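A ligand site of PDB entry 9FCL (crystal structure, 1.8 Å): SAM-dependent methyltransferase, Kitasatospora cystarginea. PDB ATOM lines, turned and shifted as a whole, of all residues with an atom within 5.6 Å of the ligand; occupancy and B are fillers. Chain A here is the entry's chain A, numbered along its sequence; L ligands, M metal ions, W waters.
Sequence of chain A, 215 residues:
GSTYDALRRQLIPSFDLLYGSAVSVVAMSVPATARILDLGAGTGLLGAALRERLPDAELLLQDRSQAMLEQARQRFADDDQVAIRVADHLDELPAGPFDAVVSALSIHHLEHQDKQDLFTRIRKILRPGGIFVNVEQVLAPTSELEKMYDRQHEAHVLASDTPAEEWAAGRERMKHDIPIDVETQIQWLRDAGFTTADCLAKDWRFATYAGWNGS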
ATOM      1  N   THR A   3      -7.117  -7.219 -35.586  1.00  0.00           N
ATOM      2  CA  THR A   3      -7.612  -6.464 -36.786  1.00  0.00           C
ATOM      3  C   THR A   3      -8.996  -6.999 -37.155  1.00  0.00           C
ATOM      4  O   THR A   3      -9.533  -7.810 -36.353  1.00  0.00           O
ATOM      5  CB  THR A   3      -6.556  -6.534 -37.892  1.00  0.00           C
ATOM      6  OG1 THR A   3      -5.268  -6.541 -37.261  1.00  0.00           O
ATOM      7  CG2 THR A   3      -6.625  -5.395 -38.877  1.00  0.00           C
ATOM      8  N   ARG A   8      -8.891 -12.046 -39.661  1.00  0.00           N
ATOM      9  CA  ARG A   8      -8.128 -12.815 -38.639  1.00  0.00           C
ATOM     10  C   ARG A   8      -8.447 -14.309 -38.745  1.00  0.00           C
ATOM     11  O   ARG A   8      -7.508 -15.124 -38.604  1.00  0.00           O
ATOM     12  CB  ARG A   8      -8.414 -12.280 -37.226  1.00  0.00           C
ATOM     13  CG  ARG A   8      -8.048 -10.819 -37.031  1.00  0.00           C
ATOM     14  CD  ARG A   8      -6.642 -10.489 -37.490  1.00  0.00           C
ATOM     15  NE  ARG A   8      -5.623 -11.176 -36.689  1.00  0.00           N
ATOM     16  CZ  ARG A   8      -4.339 -11.259 -37.001  1.00  0.00           C
ATOM     17  NH1 ARG A   8      -3.883 -10.723 -38.122  1.00  0.00           N
ATOM     18  NH2 ARG A   8      -3.504 -11.891 -36.196  1.00  0.00           N
ATOM     19  N   TYR A  19      -8.809 -19.741 -29.659  1.00  0.00           N
ATOM     20  CA  TYR A  19      -9.314 -18.609 -28.826  1.00  0.00           C
ATOM     21  C   TYR A  19     -10.353 -19.162 -27.839  1.00  0.00           C
ATOM     22  O   TYR A  19     -10.339 -18.735 -26.664  1.00  0.00           O
ATOM     23  CB  TYR A  19      -9.868 -17.471 -29.672  1.00  0.00           C
ATOM     24  CG  TYR A  19      -8.844 -16.516 -30.231  1.00  0.00           C
ATOM     25  CD1 TYR A  19      -8.725 -15.224 -29.744  1.00  0.00           C
ATOM     26  CD2 TYR A  19      -7.993 -16.891 -31.261  1.00  0.00           C
ATOM     27  CE1 TYR A  19      -7.798 -14.337 -30.268  1.00  0.00           C
ATOM     28  CE2 TYR A  19      -7.051 -16.011 -31.786  1.00  0.00           C
ATOM     29  CZ  TYR A  19      -6.949 -14.731 -31.289  1.00  0.00           C
ATOM     30  OH  TYR A  19      -6.045 -13.863 -31.827  1.00  0.00           O
ATOM     31  N   ASP A  38      -5.103  -8.440 -20.494  1.00  0.00           N
ATOM     32  CA  ASP A  38      -4.876  -8.894 -21.904  1.00  0.00           C
ATOM     33  C   ASP A  38      -3.613  -8.192 -22.414  1.00  0.00           C
ATOM     34  O   ASP A  38      -3.689  -6.966 -22.651  1.00  0.00           O
ATOM     35  CB  ASP A  38      -6.097  -8.645 -22.783  1.00  0.00           C
ATOM     36  CG  ASP A  38      -6.015  -9.213 -24.195  1.00  0.00           C
ATOM     37  OD1 ASP A  38      -5.028  -9.932 -24.495  1.00  0.00           O
ATOM     38  OD2 ASP A  38      -6.950  -8.925 -24.987  1.00  0.00           O
ATOM     39  N   LEU A  39      -2.503  -8.929 -22.521  1.00  0.00           N
ATOM     40  CA  LEU A  39      -1.176  -8.395 -22.938  1.00  0.00           C
ATOM     41  C   LEU A  39      -1.106  -8.386 -24.463  1.00  0.00           C
ATOM     42  O   LEU A  39      -1.300  -9.444 -25.069  1.00  0.00           O
ATOM     43  CB  LEU A  39      -0.049  -9.279 -22.388  1.00  0.00           C
ATOM     44  CG  LEU A  39       0.504  -8.927 -21.017  1.00  0.00           C
ATOM     45  CD1 LEU A  39       1.646  -9.882 -20.681  1.00  0.00           C
ATOM     46  CD2 LEU A  39       0.977  -7.480 -20.958  1.00  0.00           C
ATOM     47  N   GLY A  40      -0.766  -7.243 -25.064  1.00  0.00           N
ATOM     48  CA  GLY A  40      -0.739  -7.121 -26.532  1.00  0.00           C
ATOM     49  C   GLY A  40      -2.133  -7.320 -27.099  1.00  0.00           C
ATOM     50  O   GLY A  40      -2.286  -8.094 -28.060  1.00  0.00           O
ATOM     51  N   ALA A  41      -3.118  -6.666 -26.472  1.00  0.00           N
ATOM     52  CA  ALA A  41      -4.569  -6.821 -26.723  1.00  0.00           C
ATOM     53  C   ALA A  41      -4.936  -6.464 -28.174  1.00  0.00           C
ATOM     54  O   ALA A  41      -6.007  -6.919 -28.636  1.00  0.00           O
ATOM     55  CB  ALA A  41      -5.341  -5.971 -25.746  1.00  0.00           C
ATOM     56  N   GLY A  42      -4.122  -5.667 -28.868  1.00  0.00           N
ATOM     57  CA  GLY A  42      -4.435  -5.212 -30.231  1.00  0.00           C
ATOM     58  C   GLY A  42      -5.802  -4.567 -30.266  1.00  0.00           C
ATOM     59  O   GLY A  42      -6.062  -3.684 -29.419  1.00  0.00           O
ATOM     60  N   THR A  43      -6.689  -5.021 -31.164  1.00  0.00           N
ATOM     61  CA  THR A  43      -8.075  -4.510 -31.301  1.00  0.00           C
ATOM     62  C   THR A  43      -8.984  -5.139 -30.224  1.00  0.00           C
ATOM     63  O   THR A  43     -10.173  -4.811 -30.245  1.00  0.00           O
ATOM     64  CB  THR A  43      -8.635  -4.757 -32.704  1.00  0.00           C
ATOM     65  OG1 THR A  43      -8.881  -6.149 -32.873  1.00  0.00           O
ATOM     66  CG2 THR A  43      -7.708  -4.258 -33.792  1.00  0.00           C
ATOM     67  N   GLY A  44      -8.457  -5.994 -29.350  1.00  0.00           N
ATOM     68  CA  GLY A  44      -9.181  -6.530 -28.179  1.00  0.00           C
ATOM     69  C   GLY A  44      -9.970  -7.804 -28.481  1.00  0.00           C
ATOM     70  O   GLY A  44     -10.935  -8.087 -27.741  1.00  0.00           O
ATOM     71  N   LEU A  45      -9.560  -8.587 -29.477  1.00  0.00           N
ATOM     72  CA  LEU A  45     -10.292  -9.813 -29.909  1.00  0.00           C
ATOM     73  C   LEU A  45     -10.350 -10.828 -28.767  1.00  0.00           C
ATOM     74  O   LEU A  45     -11.438 -11.384 -28.539  1.00  0.00           O
ATOM     75  CB  LEU A  45      -9.629 -10.419 -31.137  1.00  0.00           C
ATOM     76  CG  LEU A  45     -10.359 -10.173 -32.455  1.00  0.00           C
ATOM     77  CD1 LEU A  45      -9.581 -10.784 -33.611  1.00  0.00           C
ATOM     78  CD2 LEU A  45     -11.780 -10.714 -32.411  1.00  0.00           C
ATOM     79  N   LEU A  46      -9.230 -11.110 -28.094  1.00  0.00           N
ATOM     80  CA  LEU A  46      -9.202 -12.099 -26.984  1.00  0.00           C
ATOM     81  C   LEU A  46     -10.016 -11.560 -25.798  1.00  0.00           C
ATOM     82  O   LEU A  46     -10.806 -12.314 -25.223  1.00  0.00           O
ATOM     83  CB  LEU A  46      -7.760 -12.428 -26.604  1.00  0.00           C
ATOM     84  CG  LEU A  46      -7.605 -13.447 -25.465  1.00  0.00           C
ATOM     85  CD1 LEU A  46      -8.429 -14.690 -25.739  1.00  0.00           C
ATOM     86  CD2 LEU A  46      -6.143 -13.813 -25.241  1.00  0.00           C
ATOM     87  N   GLN A  62      -3.909  -4.046 -22.685  1.00  0.00           N
ATOM     88  CA  GLN A  62      -2.597  -3.387 -22.755  1.00  0.00           C
ATOM     89  C   GLN A  62      -1.964  -3.670 -24.111  1.00  0.00           C
ATOM     90  O   GLN A  62      -2.031  -4.814 -24.586  1.00  0.00           O
ATOM     91  CB  GLN A  62      -1.718  -3.837 -21.592  1.00  0.00           C
ATOM     92  CG  GLN A  62      -0.340  -3.221 -21.633  1.00  0.00           C
ATOM     93  CD  GLN A  62       0.448  -3.527 -20.378  1.00  0.00           C
ATOM     94  OE1 GLN A  62       0.054  -3.157 -19.278  1.00  0.00           O
ATOM     95  NE2 GLN A  62       1.580  -4.179 -20.542  1.00  0.00           N
ATOM     96  N   ASP A  63      -1.379  -2.643 -24.728  1.00  0.00           N
ATOM     97  CA  ASP A  63      -0.677  -2.761 -26.022  1.00  0.00           C
ATOM     98  C   ASP A  63       0.234  -1.540 -26.159  1.00  0.00           C
ATOM     99  O   ASP A  63      -0.051  -0.516 -25.517  1.00  0.00           O
ATOM    100  CB  ASP A  63      -1.686  -2.871 -27.166  1.00  0.00           C
ATOM    101  CG  ASP A  63      -1.113  -3.491 -28.431  1.00  0.00           C
ATOM    102  OD1 ASP A  63      -1.440  -4.665 -28.701  1.00  0.00           O
ATOM    103  OD2 ASP A  63      -0.357  -2.797 -29.126  1.00  0.00           O
ATOM    104  N   ARG A  64       1.284  -1.647 -26.967  1.00  0.00           N
ATOM    105  CA  ARG A  64       2.197  -0.508 -27.221  1.00  0.00           C
ATOM    106  C   ARG A  64       1.588   0.415 -28.280  1.00  0.00           C
ATOM    107  O   ARG A  64       2.041   1.560 -28.362  1.00  0.00           O
ATOM    108  CB  ARG A  64       3.585  -1.005 -27.629  1.00  0.00           C
ATOM    109  CG  ARG A  64       3.661  -1.590 -29.024  1.00  0.00           C
ATOM    110  CD  ARG A  64       5.082  -1.959 -29.382  1.00  0.00           C
ATOM    111  NE  ARG A  64       5.147  -2.702 -30.629  1.00  0.00           N
ATOM    112  CZ  ARG A  64       6.209  -3.378 -31.060  1.00  0.00           C
ATOM    113  NH1 ARG A  64       6.152  -4.021 -32.222  1.00  0.00           N
ATOM    114  NH2 ARG A  64       7.317  -3.434 -30.335  1.00  0.00           N
ATOM    115  N   SER A  65       0.614  -0.067 -29.073  1.00  0.00           N
ATOM    116  CA  SER A  65       0.034   0.674 -30.223  1.00  0.00           C
ATOM    117  C   SER A  65      -1.289   1.352 -29.836  1.00  0.00           C
ATOM    118  O   SER A  65      -2.288   0.627 -29.625  1.00  0.00           O
ATOM    119  CB  SER A  65      -0.156  -0.211 -31.427  1.00  0.00           C
ATOM    120  OG  SER A  65      -0.911   0.473 -32.427  1.00  0.00           O
ATOM    121  N   MET A  68      -3.954   0.500 -32.555  1.00  0.00           N
ATOM    122  CA  MET A  68      -4.612  -0.809 -32.273  1.00  0.00           C
ATOM    123  C   MET A  68      -5.630  -0.629 -31.143  1.00  0.00           C
ATOM    124  O   MET A  68      -6.773  -1.118 -31.281  1.00  0.00           O
ATOM    125  CB  MET A  68      -3.588  -1.878 -31.902  1.00  0.00           C
ATOM    126  CG  MET A  68      -2.665  -2.275 -33.044  1.00  0.00           C
ATOM    127  SD  MET A  68      -3.500  -3.142 -34.406  1.00  0.00           S
ATOM    128  CE  MET A  68      -3.712  -4.771 -33.706  1.00  0.00           C
ATOM    129  N   ALA A  87       1.299   0.434 -23.047  1.00  0.00           N
ATOM    130  CA  ALA A  87       2.609   0.002 -22.535  1.00  0.00           C
ATOM    131  C   ALA A  87       3.203  -1.109 -23.408  1.00  0.00           C
ATOM    132  O   ALA A  87       2.436  -1.963 -23.899  1.00  0.00           O
ATOM    133  CB  ALA A  87       2.480  -0.463 -21.105  1.00  0.00           C
ATOM    134  N   ASP A  88       4.522  -1.089 -23.559  1.00  0.00           N
ATOM    135  CA  ASP A  88       5.312  -2.192 -24.156  1.00  0.00           C
ATOM    136  C   ASP A  88       5.320  -3.368 -23.169  1.00  0.00           C
ATOM    137  O   ASP A  88       5.223  -3.113 -21.950  1.00  0.00           O
ATOM    138  CB  ASP A  88       6.722  -1.712 -24.480  1.00  0.00           C
ATOM    139  CG  ASP A  88       7.396  -2.541 -25.553  1.00  0.00           C
ATOM    140  OD1 ASP A  88       7.822  -3.674 -25.226  1.00  0.00           O
ATOM    141  OD2 ASP A  88       7.458  -2.067 -26.691  1.00  0.00           O
ATOM    142  N   HIS A  89       5.460  -4.599 -23.669  1.00  0.00           N
ATOM    143  CA  HIS A  89       5.667  -5.819 -22.843  1.00  0.00           C
ATOM    144  C   HIS A  89       6.905  -5.631 -21.944  1.00  0.00           C
ATOM    145  O   HIS A  89       6.941  -6.248 -20.882  1.00  0.00           O
ATOM    146  CB  HIS A  89       5.875  -7.083 -23.685  1.00  0.00           C
ATOM    147  CG  HIS A  89       4.737  -7.447 -24.580  1.00  0.00           C
ATOM    148  ND1 HIS A  89       3.442  -7.048 -24.347  1.00  0.00           N
ATOM    149  CD2 HIS A  89       4.715  -8.204 -25.705  1.00  0.00           C
ATOM    150  CE1 HIS A  89       2.666  -7.532 -25.297  1.00  0.00           C
ATOM    151  NE2 HIS A  89       3.415  -8.251 -26.131  1.00  0.00           N
ATOM    152  N   LEU A  90       7.886  -4.844 -22.403  1.00  0.00           N
ATOM    153  CA  LEU A  90       9.170  -4.623 -21.705  1.00  0.00           C
ATOM    154  C   LEU A  90       9.060  -3.460 -20.716  1.00  0.00           C
ATOM    155  O   LEU A  90       9.989  -3.282 -19.940  1.00  0.00           O
ATOM    156  CB  LEU A  90      10.286  -4.377 -22.732  1.00  0.00           C
ATOM    157  CG  LEU A  90      10.466  -5.475 -23.780  1.00  0.00           C
ATOM    158  CD1 LEU A  90      11.692  -5.217 -24.636  1.00  0.00           C
ATOM    159  CD2 LEU A  90      10.564  -6.851 -23.127  1.00  0.00           C
ATOM    160  N   SER A 103      -2.812 -13.540 -23.456  1.00  0.00           N
ATOM    161  CA  SER A 103      -2.128 -12.937 -24.619  1.00  0.00           C
ATOM    162  C   SER A 103      -2.471 -13.750 -25.850  1.00  0.00           C
ATOM    163  O   SER A 103      -2.678 -14.975 -25.717  1.00  0.00           O
ATOM    164  CB  SER A 103      -0.635 -12.870 -24.388  1.00  0.00           C
ATOM    165  OG  SER A 103      -0.040 -11.957 -25.299  1.00  0.00           O
ATOM    166  N   ALA A 104      -2.563 -13.104 -27.003  1.00  0.00           N
ATOM    167  CA  ALA A 104      -2.741 -13.791 -28.301  1.00  0.00           C
ATOM    168  C   ALA A 104      -1.809 -13.158 -29.332  1.00  0.00           C
ATOM    169  O   ALA A 104      -1.924 -11.938 -29.537  1.00  0.00           O
ATOM    170  CB  ALA A 104      -4.189 -13.743 -28.726  1.00  0.00           C
ATOM    171  N   LEU A 105      -0.917 -13.957 -29.907  1.00  0.00           N
ATOM    172  CA  LEU A 105      -0.148 -13.641 -31.141  1.00  0.00           C
ATOM    173  C   LEU A 105       0.659 -12.354 -30.959  1.00  0.00           C
ATOM    174  O   LEU A 105       0.745 -11.562 -31.902  1.00  0.00           O
ATOM    175  CB  LEU A 105      -1.147 -13.509 -32.315  1.00  0.00           C
ATOM    176  CG  LEU A 105      -2.048 -14.720 -32.534  1.00  0.00           C
ATOM    177  CD1 LEU A 105      -2.991 -14.502 -33.712  1.00  0.00           C
ATOM    178  CD2 LEU A 105      -1.227 -15.970 -32.772  1.00  0.00           C
ATOM    179  N   SER A 106       1.291 -12.185 -29.800  1.00  0.00           N
ATOM    180  CA  SER A 106       2.014 -10.941 -29.429  1.00  0.00           C
ATOM    181  C   SER A 106       3.422 -11.276 -28.929  1.00  0.00           C
ATOM    182  O   SER A 106       4.388 -10.603 -29.339  1.00  0.00           O
ATOM    183  CB  SER A 106       1.240 -10.175 -28.386  1.00  0.00           C
ATOM    184  OG  SER A 106       1.756  -8.869 -28.260  1.00  0.00           O
ATOM    185  N   HIS A 109       6.866 -11.759 -30.809  1.00  0.00           N
ATOM    186  CA  HIS A 109       7.593 -10.552 -31.311  1.00  0.00           C
ATOM    187  C   HIS A 109       8.763 -10.189 -30.399  1.00  0.00           C
ATOM    188  O   HIS A 109       9.546  -9.328 -30.785  1.00  0.00           O
ATOM    189  CB  HIS A 109       6.629  -9.372 -31.489  1.00  0.00           C
ATOM    190  CG  HIS A 109       5.647  -9.588 -32.578  1.00  0.00           C
ATOM    191  ND1 HIS A 109       4.293  -9.640 -32.342  1.00  0.00           N
ATOM    192  CD2 HIS A 109       5.813  -9.801 -33.907  1.00  0.00           C
ATOM    193  CE1 HIS A 109       3.653  -9.846 -33.475  1.00  0.00           C
ATOM    194  NE2 HIS A 109       4.574  -9.950 -34.459  1.00  0.00           N
ATOM    195  N   LEU A 110       8.900 -10.818 -29.231  1.00  0.00           N
ATOM    196  CA  LEU A 110      10.008 -10.544 -28.280  1.00  0.00           C
ATOM    197  C   LEU A 110      11.186 -11.476 -28.574  1.00  0.00           C
ATOM    198  O   LEU A 110      10.947 -12.635 -28.967  1.00  0.00           O
ATOM    199  CB  LEU A 110       9.524 -10.738 -26.844  1.00  0.00           C
ATOM    200  CG  LEU A 110       8.418  -9.793 -26.374  1.00  0.00           C
ATOM    201  CD1 LEU A 110       8.018 -10.128 -24.948  1.00  0.00           C
ATOM    202  CD2 LEU A 110       8.857  -8.330 -26.475  1.00  0.00           C
HETATM  203  N1  LIG L   1      -4.056  -9.835 -29.276  1.00  0.00           N
HETATM  204  C1  LIG L   1      -4.687  -9.299 -30.519  1.00  0.00           C
HETATM  205  C2  LIG L   1      -5.400 -10.442 -31.266  1.00  0.00           C
HETATM  206  O1  LIG L   1      -5.381 -11.595 -30.837  1.00  0.00           O
HETATM  207  O2  LIG L   1      -5.994 -10.223 -32.320  1.00  0.00           O
HETATM  208  C3  LIG L   1      -3.656  -8.654 -31.446  1.00  0.00           C
HETATM  209  C4  LIG L   1      -2.554  -9.573 -31.967  1.00  0.00           C
HETATM  210  S1  LIG L   1      -1.529  -8.626 -33.122  1.00  0.00           S
HETATM  211  C5  LIG L   1      -1.079  -9.848 -34.341  1.00  0.00           C
HETATM  212  C6  LIG L   1      -0.039  -8.405 -32.126  1.00  0.00           C
HETATM  213  C7  LIG L   1      -0.191  -7.249 -31.141  1.00  0.00           C
HETATM  214  O3  LIG L   1       0.961  -7.209 -30.271  1.00  0.00           O
HETATM  215  C8  LIG L   1      -0.309  -5.866 -31.772  1.00  0.00           C
HETATM  216  O4  LIG L   1      -1.398  -5.157 -31.188  1.00  0.00           O
HETATM  217  C9  LIG L   1       1.035  -5.202 -31.451  1.00  0.00           C
HETATM  218  O5  LIG L   1       0.943  -3.798 -31.320  1.00  0.00           O
HETATM  219  C10 LIG L   1       1.349  -5.854 -30.111  1.00  0.00           C
HETATM  220  N2  LIG L   1       2.753  -5.850 -29.734  1.00  0.00           N
HETATM  221  C11 LIG L   1       3.805  -6.371 -30.431  1.00  0.00           C
HETATM  222  N3  LIG L   1       4.961  -6.246 -29.810  1.00  0.00           N
HETATM  223  C12 LIG L   1       4.641  -5.633 -28.612  1.00  0.00           C
HETATM  224  C13 LIG L   1       5.418  -5.224 -27.514  1.00  0.00           C
HETATM  225  N4  LIG L   1       6.732  -5.404 -27.432  1.00  0.00           N
HETATM  226  N5  LIG L   1       4.782  -4.635 -26.473  1.00  0.00           N
HETATM  227  C14 LIG L   1       3.459  -4.460 -26.556  1.00  0.00           C
HETATM  228  N6  LIG L   1       2.614  -4.795 -27.529  1.00  0.00           N
HETATM  229  C15 LIG L   1       3.281  -5.389 -28.540  1.00  0.00           C
HETATM  230 CA    CA M   1       3.512 -11.847 -35.784  1.00  0.00          CA
HETATM  231  O   HOH W   1      -3.522 -10.335 -26.556  1.00  0.00           O
HETATM  232  O   HOH W   2      -5.918 -12.187 -34.087  1.00  0.00           O
HETATM  233  O   HOH W   3       2.775  -2.565 -32.916  1.00  0.00           O
HETATM  234  O   HOH W   4      -6.635  -9.365 -27.634  1.00  0.00           O
HETATM  235  O   HOH W   5      -6.679  -7.470 -32.806  1.00  0.00           O
HETATM  236  O   HOH W   6       1.273 -11.344 -34.846  1.00  0.00           O
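O4 of the ligand lies within hydrogen-bond range of OD1 of Asp 63, 2.5 Å away.
O1 of the ligand lies within hydrogen-bond range of OH of Tyr 19, 2.6 Å away.
An oxygen (O3) of the ligand sits at hydrogen-bond distance from the side-chain hydroxyl (OG) of Ser 106 (2.7 Å).
N1 of the ligand sits at hydrogen-bond distance from O of Gly 40, at 2.8 Å.
N of His 89 is in hydrogen-bond range of N5 of the ligand (2.9 Å).
A ring nitrogen (ND1) of His 89 lies close to a nitrogen (N5) of the ligand.
N1 of the ligand is in hydrogen-bond range of O of Ala 104 (3.0 Å).
OD1 of Asp 88 sits at hydrogen-bond distance from N4 of the ligand, 3.0 Å away.
The backbone NH (N) of Arg 64 is in hydrogen-bond range of a nitrogen (N6) of the ligand, at 3.5 Å.
The guanidinium group of Arg 64 lies close to a nitrogen (N3) of the ligand.
Water W2 lies within hydrogen-bond range of O2 of the ligand (2.6 Å), NE of Arg 8 (2.8 Å) and OH of Tyr 19 (2.8 Å).
Water W3 bridges O5 of the ligand (2.7 Å) and NE of Arg 64 (3.3 Å).
Water W5 lies within hydrogen-bond range of OG1 of Thr 43, N of Thr 3 and O2 of the ligand.
Water W4 lies within hydrogen-bond range of OD2 of Asp 38 (2.7 Å), O of Ala 41 (2.7 Å), N1 of the ligand (3.1 Å) and N of Leu 46 (3.2 Å).
OD1 of Asp 63 lies within hydrogen-bond range of N of Gly 42.
The side-chain carboxylate (OD1) of Asp 63 sits at hydrogen-bond distance from the backbone NH (N) of Ala 41 (3.4 Å).
O of Ser 106 is in hydrogen-bond range of ND1 of His 109, at 3.2 Å.
The backbone NH of Gly 40 sits at hydrogen-bond distance from the backbone carbonyl oxygen of Gln 62 (2.8 Å).
OD2 of Asp 88 is in salt-bridge range of NH2 of Arg 64 (3.9 Å).
The side-chain carboxylate (OD1) of Asp 88 lies within hydrogen-bond range of the backbone NH (N) of Leu 90 (3.1 Å).
The backbone NH (N) of Ala 41 is in hydrogen-bond range of the backbone carbonyl oxygen (O) of Gln 62 (2.9 Å).
N of Met 68 lies within hydrogen-bond range of OG of Ser 65 (3.0 Å).
Merely in contact with the ligand: Gly 42 (3.2 Å), Leu 105 (3.3 Å), Ala 41 (3.3 Å), Met 68 (3.4 Å), Arg 8 (3.7 Å), Leu 110 (3.7 Å), Ser 65 (3.8 Å), Ala 87 (3.8 Å), His 109 (3.8 Å) and Leu 45 (3.8 Å).
Hydrophobic or aromatic side chains within 4 Å of the ligand: Tyr 19, Leu 45, Met 68, His 89, Ala 104, His 109 and Leu 110.
18 residues have an atom within 4 Å of the ligand: Arg 8, Tyr 19, Gly 40, Ala 41, Gly 42, Leu 45, Asp 63, Arg 64, Ser 65, Met 68, Ala 87, Asp 88, His 89, Ala 104, Leu 105, Ser 106, His 109 and Leu 110.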
